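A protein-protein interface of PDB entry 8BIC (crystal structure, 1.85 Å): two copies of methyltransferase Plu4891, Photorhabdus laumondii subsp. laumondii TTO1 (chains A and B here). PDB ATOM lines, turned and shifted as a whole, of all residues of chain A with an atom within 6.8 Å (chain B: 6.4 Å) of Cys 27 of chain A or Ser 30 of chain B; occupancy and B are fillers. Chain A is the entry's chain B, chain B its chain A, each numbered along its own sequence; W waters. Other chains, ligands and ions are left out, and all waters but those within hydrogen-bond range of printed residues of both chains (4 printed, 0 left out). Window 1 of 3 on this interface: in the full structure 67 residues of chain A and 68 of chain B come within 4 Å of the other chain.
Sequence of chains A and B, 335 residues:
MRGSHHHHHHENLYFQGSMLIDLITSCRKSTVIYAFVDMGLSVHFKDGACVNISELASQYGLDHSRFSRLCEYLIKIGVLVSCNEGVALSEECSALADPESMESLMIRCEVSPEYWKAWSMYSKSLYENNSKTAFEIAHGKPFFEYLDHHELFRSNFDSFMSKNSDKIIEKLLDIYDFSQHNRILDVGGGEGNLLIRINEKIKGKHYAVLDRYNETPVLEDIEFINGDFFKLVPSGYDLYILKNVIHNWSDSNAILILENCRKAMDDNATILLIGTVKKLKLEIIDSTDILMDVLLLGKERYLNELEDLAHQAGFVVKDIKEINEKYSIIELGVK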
ATOM      1  N   ASP A  22      13.762   8.075 -17.550  1.00  0.00           N
ATOM      2  CA  ASP A  22      13.468   7.284 -16.325  1.00  0.00           C
ATOM      3  C   ASP A  22      14.436   7.684 -15.202  1.00  0.00           C
ATOM      4  O   ASP A  22      13.969   7.903 -14.067  1.00  0.00           O
ATOM      5  CB  ASP A  22      13.528   5.777 -16.573  1.00  0.00           C
ATOM      6  CG  ASP A  22      13.236   4.984 -15.312  1.00  0.00           C
ATOM      7  OD1 ASP A  22      12.085   5.054 -14.829  1.00  0.00           O
ATOM      8  OD2 ASP A  22      14.167   4.340 -14.799  1.00  0.00           O
ATOM      9  N   LEU A  23      15.738   7.752 -15.487  1.00  0.00           N
ATOM     10  CA  LEU A  23      16.761   8.149 -14.483  1.00  0.00           C
ATOM     11  C   LEU A  23      16.492   9.591 -14.037  1.00  0.00           C
ATOM     12  O   LEU A  23      16.518   9.848 -12.821  1.00  0.00           O
ATOM     13  CB  LEU A  23      18.166   8.021 -15.078  1.00  0.00           C
ATOM     14  CG  LEU A  23      18.656   6.603 -15.377  1.00  0.00           C
ATOM     15  CD1 LEU A  23      20.046   6.653 -15.988  1.00  0.00           C
ATOM     16  CD2 LEU A  23      18.671   5.736 -14.126  1.00  0.00           C
ATOM     17  N   ILE A  24      16.246  10.491 -14.993  1.00  0.00           N
ATOM     18  CA  ILE A  24      16.022  11.946 -14.733  1.00  0.00           C
ATOM     19  C   ILE A  24      14.811  12.106 -13.805  1.00  0.00           C
ATOM     20  O   ILE A  24      14.899  12.946 -12.904  1.00  0.00           O
ATOM     21  CB  ILE A  24      15.873  12.739 -16.049  1.00  0.00           C
ATOM     22  CG1 ILE A  24      17.230  12.906 -16.739  1.00  0.00           C
ATOM     23  CG2 ILE A  24      15.199  14.085 -15.809  1.00  0.00           C
ATOM     24  CD1 ILE A  24      17.150  13.451 -18.141  1.00  0.00           C
ATOM     25  N   THR A  25      13.761  11.300 -13.988  1.00  0.00           N
ATOM     26  CA  THR A  25      12.467  11.415 -13.251  1.00  0.00           C
ATOM     27  C   THR A  25      12.434  10.471 -12.045  1.00  0.00           C
ATOM     28  O   THR A  25      11.361  10.376 -11.427  1.00  0.00           O
ATOM     29  CB  THR A  25      11.259  11.176 -14.170  1.00  0.00           C
ATOM     30  OG1 THR A  25      11.299   9.860 -14.733  1.00  0.00           O
ATOM     31  CG2 THR A  25      11.177  12.210 -15.270  1.00  0.00           C
ATOM     32  N   SER A  26      13.556   9.823 -11.707  1.00  0.00           N
ATOM     33  CA  SER A  26      13.675   8.871 -10.568  1.00  0.00           C
ATOM     34  C   SER A  26      13.168   9.506  -9.261  1.00  0.00           C
ATOM     35  O   SER A  26      12.570   8.790  -8.441  1.00  0.00           O
ATOM     36  CB  SER A  26      15.093   8.389 -10.423  1.00  0.00           C
ATOM     37  OG  SER A  26      15.484   7.638 -11.559  1.00  0.00           O
ATOM     38  N   CYS A  27      13.410  10.803  -9.067  1.00  0.00           N
ATOM     39  CA  CYS A  27      13.036  11.546  -7.833  1.00  0.00           C
ATOM     40  C   CYS A  27      11.513  11.505  -7.608  1.00  0.00           C
ATOM     41  O   CYS A  27      11.106  11.581  -6.442  1.00  0.00           O
ATOM     42  CB  CYS A  27      13.524  12.986  -7.888  1.00  0.00           C
ATOM     43  SG  CYS A  27      13.008  13.867  -9.381  1.00  0.00           S
ATOM     44  N   ARG A  28      10.715  11.377  -8.675  1.00  0.00           N
ATOM     45  CA  ARG A  28       9.230  11.264  -8.611  1.00  0.00           C
ATOM     46  C   ARG A  28       8.820  10.054  -7.763  1.00  0.00           C
ATOM     47  O   ARG A  28       7.791  10.148  -7.063  1.00  0.00           O
ATOM     48  CB  ARG A  28       8.619  11.187 -10.012  1.00  0.00           C
ATOM     49  CG  ARG A  28       8.855  12.433 -10.851  1.00  0.00           C
ATOM     50  CD  ARG A  28       8.185  12.348 -12.205  1.00  0.00           C
ATOM     51  NE  ARG A  28       8.613  13.411 -13.104  1.00  0.00           N
ATOM     52  CZ  ARG A  28       8.152  13.591 -14.339  1.00  0.00           C
ATOM     53  NH1 ARG A  28       8.600  14.594 -15.071  1.00  0.00           N
ATOM     54  NH2 ARG A  28       7.249  12.768 -14.844  1.00  0.00           N
ATOM     55  N   LYS A  29       9.607   8.978  -7.782  1.00  0.00           N
ATOM     56  CA  LYS A  29       9.354   7.767  -6.953  1.00  0.00           C
ATOM     57  C   LYS A  29       9.539   8.106  -5.466  1.00  0.00           C
ATOM     58  O   LYS A  29       8.690   7.690  -4.645  1.00  0.00           O
ATOM     59  CB  LYS A  29      10.276   6.614  -7.354  1.00  0.00           C
ATOM     60  CG  LYS A  29      10.160   6.167  -8.806  1.00  0.00           C
ATOM     61  CD  LYS A  29      10.863   4.851  -9.074  1.00  0.00           C
ATOM     62  CE  LYS A  29      11.936   4.987 -10.126  1.00  0.00           C
ATOM     63  NZ  LYS A  29      12.634   3.699 -10.356  1.00  0.00           N
ATOM     64  N   SER A  30      10.613   8.825  -5.125  1.00  0.00           N
ATOM     65  CA  SER A  30      10.883   9.283  -3.734  1.00  0.00           C
ATOM     66  C   SER A  30       9.727  10.181  -3.262  1.00  0.00           C
ATOM     67  O   SER A  30       9.220   9.982  -2.127  1.00  0.00           O
ATOM     68  CB  SER A  30      12.219   9.987  -3.632  1.00  0.00           C
ATOM     69  OG  SER A  30      13.298   9.113  -3.995  1.00  0.00           O
ATOM     70  N   THR A  31       9.296  11.130  -4.095  1.00  0.00           N
ATOM     71  CA  THR A  31       8.318  12.162  -3.663  1.00  0.00           C
ATOM     72  C   THR A  31       6.922  11.542  -3.526  1.00  0.00           C
ATOM     73  O   THR A  31       6.205  11.966  -2.612  1.00  0.00           O
ATOM     74  CB  THR A  31       8.362  13.417  -4.540  1.00  0.00           C
ATOM     75  OG1 THR A  31       8.234  13.049  -5.908  1.00  0.00           O
ATOM     76  CG2 THR A  31       9.628  14.221  -4.324  1.00  0.00           C
ATOM     77  N   VAL A  32       6.552  10.539  -4.334  1.00  0.00           N
ATOM     78  CA  VAL A  32       5.211   9.903  -4.163  1.00  0.00           C
ATOM     79  C   VAL A  32       5.241   9.025  -2.914  1.00  0.00           C
ATOM     80  O   VAL A  32       4.209   8.980  -2.213  1.00  0.00           O
ATOM     81  CB  VAL A  32       4.696   9.149  -5.403  1.00  0.00           C
ATOM     82  CG1 VAL A  32       4.460  10.136  -6.530  1.00  0.00           C
ATOM     83  CG2 VAL A  32       5.603   8.002  -5.833  1.00  0.00           C
ATOM     84  N   TYR A  73       0.162   4.854  -9.744  1.00  0.00           N
ATOM     85  CA  TYR A  73       1.620   5.091  -9.902  1.00  0.00           C
ATOM     86  C   TYR A  73       2.392   4.243  -8.880  1.00  0.00           C
ATOM     87  O   TYR A  73       3.437   3.650  -9.248  1.00  0.00           O
ATOM     88  CB  TYR A  73       1.955   6.577  -9.804  1.00  0.00           C
ATOM     89  CG  TYR A  73       3.416   6.904  -9.991  1.00  0.00           C
ATOM     90  CD1 TYR A  73       4.042   7.813  -9.156  1.00  0.00           C
ATOM     91  CD2 TYR A  73       4.181   6.314 -10.984  1.00  0.00           C
ATOM     92  CE1 TYR A  73       5.377   8.144  -9.314  1.00  0.00           C
ATOM     93  CE2 TYR A  73       5.524   6.625 -11.148  1.00  0.00           C
ATOM     94  CZ  TYR A  73       6.127   7.542 -10.306  1.00  0.00           C
ATOM     95  OH  TYR A  73       7.444   7.886 -10.445  1.00  0.00           O
ATOM     96  N   VAL A 111      13.874  13.467   1.249  1.00  0.00           N
ATOM     97  CA  VAL A 111      13.280  14.525   0.374  1.00  0.00           C
ATOM     98  C   VAL A 111      12.990  15.786   1.203  1.00  0.00           C
ATOM     99  O   VAL A 111      12.200  16.619   0.747  1.00  0.00           O
ATOM    100  CB  VAL A 111      12.044  14.012  -0.394  1.00  0.00           C
ATOM    101  CG1 VAL A 111      12.398  12.816  -1.257  1.00  0.00           C
ATOM    102  CG2 VAL A 111      10.871  13.696   0.513  1.00  0.00           C
ATOM    103  N   TRP A 116      17.449  18.410  -0.402  1.00  0.00           N
ATOM    104  CA  TRP A 116      17.225  18.970  -1.763  1.00  0.00           C
ATOM    105  C   TRP A 116      18.210  20.120  -2.000  1.00  0.00           C
ATOM    106  O   TRP A 116      18.915  20.098  -3.018  1.00  0.00           O
ATOM    107  CB  TRP A 116      15.780  19.446  -1.941  1.00  0.00           C
ATOM    108  CG  TRP A 116      14.786  18.377  -2.274  1.00  0.00           C
ATOM    109  CD1 TRP A 116      13.696  18.011  -1.538  1.00  0.00           C
ATOM    110  CD2 TRP A 116      14.752  17.569  -3.462  1.00  0.00           C
ATOM    111  NE1 TRP A 116      13.000  17.016  -2.176  1.00  0.00           N
ATOM    112  CE2 TRP A 116      13.619  16.729  -3.361  1.00  0.00           C
ATOM    113  CE3 TRP A 116      15.564  17.471  -4.598  1.00  0.00           C
ATOM    114  CZ2 TRP A 116      13.300  15.790  -4.340  1.00  0.00           C
ATOM    115  CZ3 TRP A 116      15.251  16.543  -5.560  1.00  0.00           C
ATOM    116  CH2 TRP A 116      14.132  15.721  -5.433  1.00  0.00           C
ATOM    117  N   SER B  26      15.652   6.785  -4.706  1.00  0.00           N
ATOM    118  CA  SER B  26      15.568   7.014  -6.175  1.00  0.00           C
ATOM    119  C   SER B  26      15.991   8.442  -6.532  1.00  0.00           C
ATOM    120  O   SER B  26      16.669   8.606  -7.558  1.00  0.00           O
ATOM    121  CB  SER B  26      14.195   6.726  -6.703  1.00  0.00           C
ATOM    122  OG  SER B  26      13.881   5.356  -6.555  1.00  0.00           O
ATOM    123  N   CYS B  27      15.625   9.439  -5.717  1.00  0.00           N
ATOM    124  CA  CYS B  27      15.947  10.877  -5.965  1.00  0.00           C
ATOM    125  C   CYS B  27      17.455  11.094  -6.152  1.00  0.00           C
ATOM    126  O   CYS B  27      17.812  12.054  -6.857  1.00  0.00           O
ATOM    127  CB  CYS B  27      15.438  11.776  -4.841  1.00  0.00           C
ATOM    128  SG  CYS B  27      15.904  11.177  -3.199  1.00  0.00           S
ATOM    129  N   ARG B  28      18.304  10.275  -5.525  1.00  0.00           N
ATOM    130  CA  ARG B  28      19.794  10.411  -5.592  1.00  0.00           C
ATOM    131  C   ARG B  28      20.279  10.232  -7.041  1.00  0.00           C
ATOM    132  O   ARG B  28      21.307  10.830  -7.408  1.00  0.00           O
ATOM    133  CB  ARG B  28      20.474   9.419  -4.645  1.00  0.00           C
ATOM    134  CG  ARG B  28      20.150   9.638  -3.173  1.00  0.00           C
ATOM    135  CD  ARG B  28      20.843   8.626  -2.289  1.00  0.00           C
ATOM    136  NE  ARG B  28      20.347   8.631  -0.921  1.00  0.00           N
ATOM    137  CZ  ARG B  28      20.800   7.838   0.044  1.00  0.00           C
ATOM    138  NH1 ARG B  28      20.288   7.920   1.258  1.00  0.00           N
ATOM    139  NH2 ARG B  28      21.772   6.973  -0.204  1.00  0.00           N
ATOM    140  N   LYS B  29      19.569   9.450  -7.851  1.00  0.00           N
ATOM    141  CA  LYS B  29      19.873   9.306  -9.299  1.00  0.00           C
ATOM    142  C   LYS B  29      19.631  10.649 -10.004  1.00  0.00           C
ATOM    143  O   LYS B  29      20.503  11.090 -10.773  1.00  0.00           O
ATOM    144  CB  LYS B  29      19.041   8.181  -9.913  1.00  0.00           C
ATOM    145  CG  LYS B  29      19.257   6.808  -9.290  1.00  0.00           C
ATOM    146  CD  LYS B  29      18.695   5.686 -10.136  1.00  0.00           C
ATOM    147  CE  LYS B  29      17.797   4.763  -9.347  1.00  0.00           C
ATOM    148  NZ  LYS B  29      17.073   3.824 -10.227  1.00  0.00           N
ATOM    149  N   SER B  30      18.499  11.297  -9.736  1.00  0.00           N
ATOM    150  CA  SER B  30      18.130  12.592 -10.359  1.00  0.00           C
ATOM    151  C   SER B  30      19.152  13.668  -9.955  1.00  0.00           C
ATOM    152  O   SER B  30      19.557  14.455 -10.825  1.00  0.00           O
ATOM    153  CB  SER B  30      16.723  12.999  -9.989  1.00  0.00           C
ATOM    154  OG  SER B  30      15.767  12.075 -10.473  1.00  0.00           O
ATOM    155  N   THR B  31      19.571  13.700  -8.687  1.00  0.00           N
ATOM    156  CA  THR B  31      20.428  14.786  -8.141  1.00  0.00           C
ATOM    157  C   THR B  31      21.862  14.645  -8.670  1.00  0.00           C
ATOM    158  O   THR B  31      22.474  15.686  -8.955  1.00  0.00           O
ATOM    159  CB  THR B  31      20.334  14.856  -6.612  1.00  0.00           C
ATOM    160  OG1 THR B  31      20.643  13.581  -6.044  1.00  0.00           O
ATOM    161  CG2 THR B  31      18.963  15.309  -6.150  1.00  0.00           C
ATOM    162  N   VAL B  32      22.393  13.429  -8.830  1.00  0.00           N
ATOM    163  CA  VAL B  32      23.774  13.257  -9.383  1.00  0.00           C
ATOM    164  C   VAL B  32      23.757  13.606 -10.877  1.00  0.00           C
ATOM    165  O   VAL B  32      24.731  14.222 -11.342  1.00  0.00           O
ATOM    166  CB  VAL B  32      24.396  11.874  -9.090  1.00  0.00           C
ATOM    167  CG1 VAL B  32      24.498  11.641  -7.587  1.00  0.00           C
ATOM    168  CG2 VAL B  32      23.681  10.720  -9.779  1.00  0.00           C
ATOM    169  N   ILE B  33      22.690  13.274 -11.609  1.00  0.00           N
ATOM    170  CA  ILE B  33      22.565  13.671 -13.045  1.00  0.00           C
ATOM    171  C   ILE B  33      22.504  15.202 -13.127  1.00  0.00           C
ATOM    172  O   ILE B  33      23.192  15.774 -13.988  1.00  0.00           O
ATOM    173  CB  ILE B  33      21.371  12.989 -13.736  1.00  0.00           C
ATOM    174  CG1 ILE B  33      21.592  11.480 -13.856  1.00  0.00           C
ATOM    175  CG2 ILE B  33      21.104  13.627 -15.093  1.00  0.00           C
ATOM    176  CD1 ILE B  33      20.384  10.700 -14.322  1.00  0.00           C
ATOM    177  N   TYR B  34      21.735  15.854 -12.255  1.00  0.00           N
ATOM    178  CA  TYR B  34      21.693  17.338 -12.170  1.00  0.00           C
ATOM    179  C   TYR B  34      23.113  17.884 -11.969  1.00  0.00           C
ATOM    180  O   TYR B  34      23.523  18.784 -12.729  1.00  0.00           O
ATOM    181  CB  TYR B  34      20.765  17.824 -11.051  1.00  0.00           C
ATOM    182  CG  TYR B  34      20.802  19.321 -10.879  1.00  0.00           C
ATOM    183  CD1 TYR B  34      21.719  19.923 -10.030  1.00  0.00           C
ATOM    184  CD2 TYR B  34      19.965  20.139 -11.620  1.00  0.00           C
ATOM    185  CE1 TYR B  34      21.768  21.302  -9.884  1.00  0.00           C
ATOM    186  CE2 TYR B  34      20.008  21.518 -11.493  1.00  0.00           C
ATOM    187  CZ  TYR B  34      20.911  22.099 -10.622  1.00  0.00           C
ATOM    188  OH  TYR B  34      20.936  23.455 -10.508  1.00  0.00           O
ATOM    189  N   ALA B  35      23.831  17.355 -10.972  1.00  0.00           N
ATOM    190  CA  ALA B  35      25.199  17.782 -10.591  1.00  0.00           C
ATOM    191  C   ALA B  35      26.136  17.652 -11.801  1.00  0.00           C
ATOM    192  O   ALA B  35      26.880  18.607 -12.083  1.00  0.00           O
ATOM    193  CB  ALA B  35      25.685  16.976  -9.409  1.00  0.00           C
ATOM    194  N   ILE B  77      24.738   3.423 -12.020  1.00  0.00           N
ATOM    195  CA  ILE B  77      23.312   3.702 -12.387  1.00  0.00           C
ATOM    196  C   ILE B  77      23.163   3.777 -13.913  1.00  0.00           C
ATOM    197  O   ILE B  77      22.018   3.914 -14.368  1.00  0.00           O
ATOM    198  CB  ILE B  77      22.771   4.966 -11.688  1.00  0.00           C
ATOM    199  CG1 ILE B  77      23.431   6.251 -12.199  1.00  0.00           C
ATOM    200  CG2 ILE B  77      22.897   4.811 -10.178  1.00  0.00           C
ATOM    201  CD1 ILE B  77      22.686   7.520 -11.840  1.00  0.00           C
ATOM    202  N   ILE B 107      16.134  17.954 -16.547  1.00  0.00           N
ATOM    203  CA  ILE B 107      16.687  17.654 -15.188  1.00  0.00           C
ATOM    204  C   ILE B 107      16.766  18.953 -14.371  1.00  0.00           C
ATOM    205  O   ILE B 107      16.523  18.884 -13.149  1.00  0.00           O
ATOM    206  CB  ILE B 107      18.040  16.910 -15.250  1.00  0.00           C
ATOM    207  CG1 ILE B 107      18.510  16.449 -13.868  1.00  0.00           C
ATOM    208  CG2 ILE B 107      19.110  17.742 -15.936  1.00  0.00           C
ATOM    209  CD1 ILE B 107      17.631  15.410 -13.229  1.00  0.00           C
ATOM    210  N   GLU B 110      13.306  19.368 -13.096  1.00  0.00           N
ATOM    211  CA  GLU B 110      12.930  18.201 -12.254  1.00  0.00           C
ATOM    212  C   GLU B 110      13.372  18.381 -10.790  1.00  0.00           C
ATOM    213  O   GLU B 110      12.578  18.043  -9.893  1.00  0.00           O
ATOM    214  CB  GLU B 110      13.549  16.935 -12.848  1.00  0.00           C
ATOM    215  CG  GLU B 110      12.859  15.670 -12.416  1.00  0.00           C
ATOM    216  CD  GLU B 110      11.418  15.516 -12.871  1.00  0.00           C
ATOM    217  OE1 GLU B 110      11.055  16.052 -13.939  1.00  0.00           O
ATOM    218  OE2 GLU B 110      10.660  14.860 -12.143  1.00  0.00           O
ATOM    219  N   VAL B 111      14.604  18.840 -10.542  1.00  0.00           N
ATOM    220  CA  VAL B 111      15.161  18.963  -9.156  1.00  0.00           C
ATOM    221  C   VAL B 111      15.304  20.447  -8.787  1.00  0.00           C
ATOM    222  O   VAL B 111      16.049  20.747  -7.860  1.00  0.00           O
ATOM    223  CB  VAL B 111      16.476  18.173  -8.986  1.00  0.00           C
ATOM    224  CG1 VAL B 111      16.274  16.692  -9.263  1.00  0.00           C
ATOM    225  CG2 VAL B 111      17.602  18.709  -9.844  1.00  0.00           C
ATOM    226  N   TRP B 119       6.216  19.429  -4.557  1.00  0.00           N
ATOM    227  CA  TRP B 119       6.095  18.012  -4.117  1.00  0.00           C
ATOM    228  C   TRP B 119       5.845  17.919  -2.604  1.00  0.00           C
ATOM    229  O   TRP B 119       5.031  17.083  -2.195  1.00  0.00           O
ATOM    230  CB  TRP B 119       7.341  17.205  -4.519  1.00  0.00           C
ATOM    231  CG  TRP B 119       7.315  16.700  -5.929  1.00  0.00           C
ATOM    232  CD1 TRP B 119       8.074  17.133  -6.980  1.00  0.00           C
ATOM    233  CD2 TRP B 119       6.492  15.637  -6.441  1.00  0.00           C
ATOM    234  NE1 TRP B 119       7.768  16.419  -8.109  1.00  0.00           N
ATOM    235  CE2 TRP B 119       6.811  15.487  -7.806  1.00  0.00           C
ATOM    236  CE3 TRP B 119       5.545  14.778  -5.874  1.00  0.00           C
ATOM    237  CZ2 TRP B 119       6.207  14.519  -8.610  1.00  0.00           C
ATOM    238  CZ3 TRP B 119       4.944  13.827  -6.669  1.00  0.00           C
ATOM    239  CH2 TRP B 119       5.261  13.714  -8.020  1.00  0.00           C
HETATM  240  O   HOH W   1      10.527  14.635  -7.565  1.00  0.00           O
HETATM  241  O   HOH W   2       5.716  14.474  -1.923  1.00  0.00           O
HETATM  242  O   HOH W   3      14.763   5.181 -11.782  1.00  0.00           O
HETATM  243  O   HOH W   4      14.815   3.462  -8.387  1.00  0.00           O
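The backbone carbonyl oxygen (O) of Cys 27 of chain B is in hydrogen-bond range of the side-chain hydroxyl (OG1) of Thr 31 of chain B, 3.3 Å away. O of Arg 28 of chain B lies within hydrogen-bond range of OG1 of Thr 31 of chain B. The side-chain hydroxyl (OG) of Ser 26 of chain A is in hydrogen-bond range of the backbone carbonyl oxygen (O) of Asp 22 of chain A, at 2.9 Å. The backbone carbonyl oxygen (O) of Leu 23 of chain A lies within hydrogen-bond range of the side-chain hydroxyl (OG) of Ser 26 of chain A, at 2.7 Å. The backbone carbonyl oxygen of Arg 28 of chain A lies within hydrogen-bond range of the side-chain hydroxyl of Thr 31 of chain A. The indole nitrogen (NE1) of Trp 116 of chain A lies within hydrogen-bond range of the backbone carbonyl oxygen (O) of Val 111 of chain A, 3.1 Å away.
Of the 14 printed residues of chain A, 10 touch a printed residue of chain B. Hydrophobic or aromatic side chains of chain B within 4 Å of the printed part of chain A: Ile 33, Ile 107, Val 111 and Trp 119. Among the printed residues, Asp or Glu carboxylates within 4 Å of a Lys or Arg side-chain nitrogen of the other chain: Arg 28 of chain A with Glu 110 of chain B.
Ser 26 of chain B touches its own counterpart, Ser 26 of chain A. Ser 26 of chain A touches Lys 29 of chain B, and with the chains exchanged Lys 29 of chain A touches Ser 26 of chain B. Ser 26 of chain A touches Ser 30 of chain B, and with the chains exchanged Ser 30 of chain A touches Ser 26 of chain B. Cys 27 of chain B touches its own counterpart, Cys 27 of chain A. 8 positions are printed for both chains.
The side-chain hydroxyl (OG) of Ser 30 of chain A is in hydrogen-bond range of the backbone NH (N) of Ser 26 of chain B, at 3.4 Å. N of Cys 27 of chain B sits at hydrogen-bond distance from OG of Ser 30 of chain A (2.9 Å). The side-chain hydroxyl (OG) of Ser 30 of chain B sits at hydrogen-bond distance from the backbone carbonyl oxygen (O) of Leu 23 of chain A (3.3 Å). OG of Ser 30 of chain B lies within hydrogen-bond range of O of Ile 24 of chain A, at 2.7 Å. The side-chain hydroxyl of Ser 30 of chain B is in hydrogen-bond range of the backbone NH of Ser 26 of chain A, at 3.4 Å. The side-chain hydroxyl (OG) of Ser 30 of chain B sits at hydrogen-bond distance from the backbone NH (N) of Cys 27 of chain A (3.0 Å). The side-chain carboxylate of Glu 110 of chain B sits close to the side-chain sulfur of Cys 27 of chain A, 3.8 Å away. The side-chain carboxylate (OE2) of Glu 110 of chain B is in salt-bridge range of the guanidinium group (NE) of Arg 28 of chain A, at 2.7 Å.
Asp 22 of chain A touches none of the printed residues of chain B. Val 111 of chain A touches none of the printed residues of chain B. Printed residues of chain A within 4 Å of Ile 33 of chain B: Leu 23 (3.6 Å). Of the printed residues of chain A, Ile 107 of chain B touches Ile 24 (3.7 Å). Printed residues of chain A within 4 Å of Val 111 of chain B: Trp 116 (3.8 Å).
Among the printed residues, pairs that only touch across the chains: Ser 26 of chain A with Ser 26 of chain B (3.1 Å), Thr 31 of chain A with Trp 119 of chain B (3.2 Å), Ile 24 of chain A with Glu 110 of chain B (3.4 Å), Cys 27 of chain A with Cys 27 of chain B (3.5 Å), Leu 23 of chain A with Ile 33 of chain B (3.6 Å), Ile 24 of chain A with Ile 107 of chain B (3.7 Å), Val 32 of chain A with Trp 119 of chain B (3.7 Å), Leu 23 of chain A with Ile 77 of chain B (3.7 Å), Trp 116 of chain A with Val 111 of chain B (3.8 Å), Lys 29 of chain A with Ser 26 of chain B (3.9 Å), Trp 116 of chain A with Thr 31 of chain B (3.96 Å), Ser 26 of chain A with Lys 29 of chain B (3.96 Å) and Leu 23 of chain A with Lys 29 of chain B (3.99 Å).
Water W3 lies within hydrogen-bond range of OG of Ser 26 of chain A (2.6 Å), NZ of Lys 29 of chain A (3.0 Å), NZ of Lys 29 of chain B (3.1 Å) and OD2 of Asp 22 of chain A (3.2 Å). Water W2 lies within hydrogen-bond range of O of Thr 31 of chain A (2.6 Å) and O of Trp 119 of chain B (2.7 Å). Water W4 lies within hydrogen-bond range of OG of Ser 26 of chain B (2.8 Å), NZ of Lys 29 of chain B (2.9 Å) and NZ of Lys 29 of chain A (2.9 Å). Water W1 lies within hydrogen-bond range of SG of Cys 27 of chain A, OG1 of Thr 31 of chain A, NE1 of Trp 119 of chain B and N of Arg 28 of chain A.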
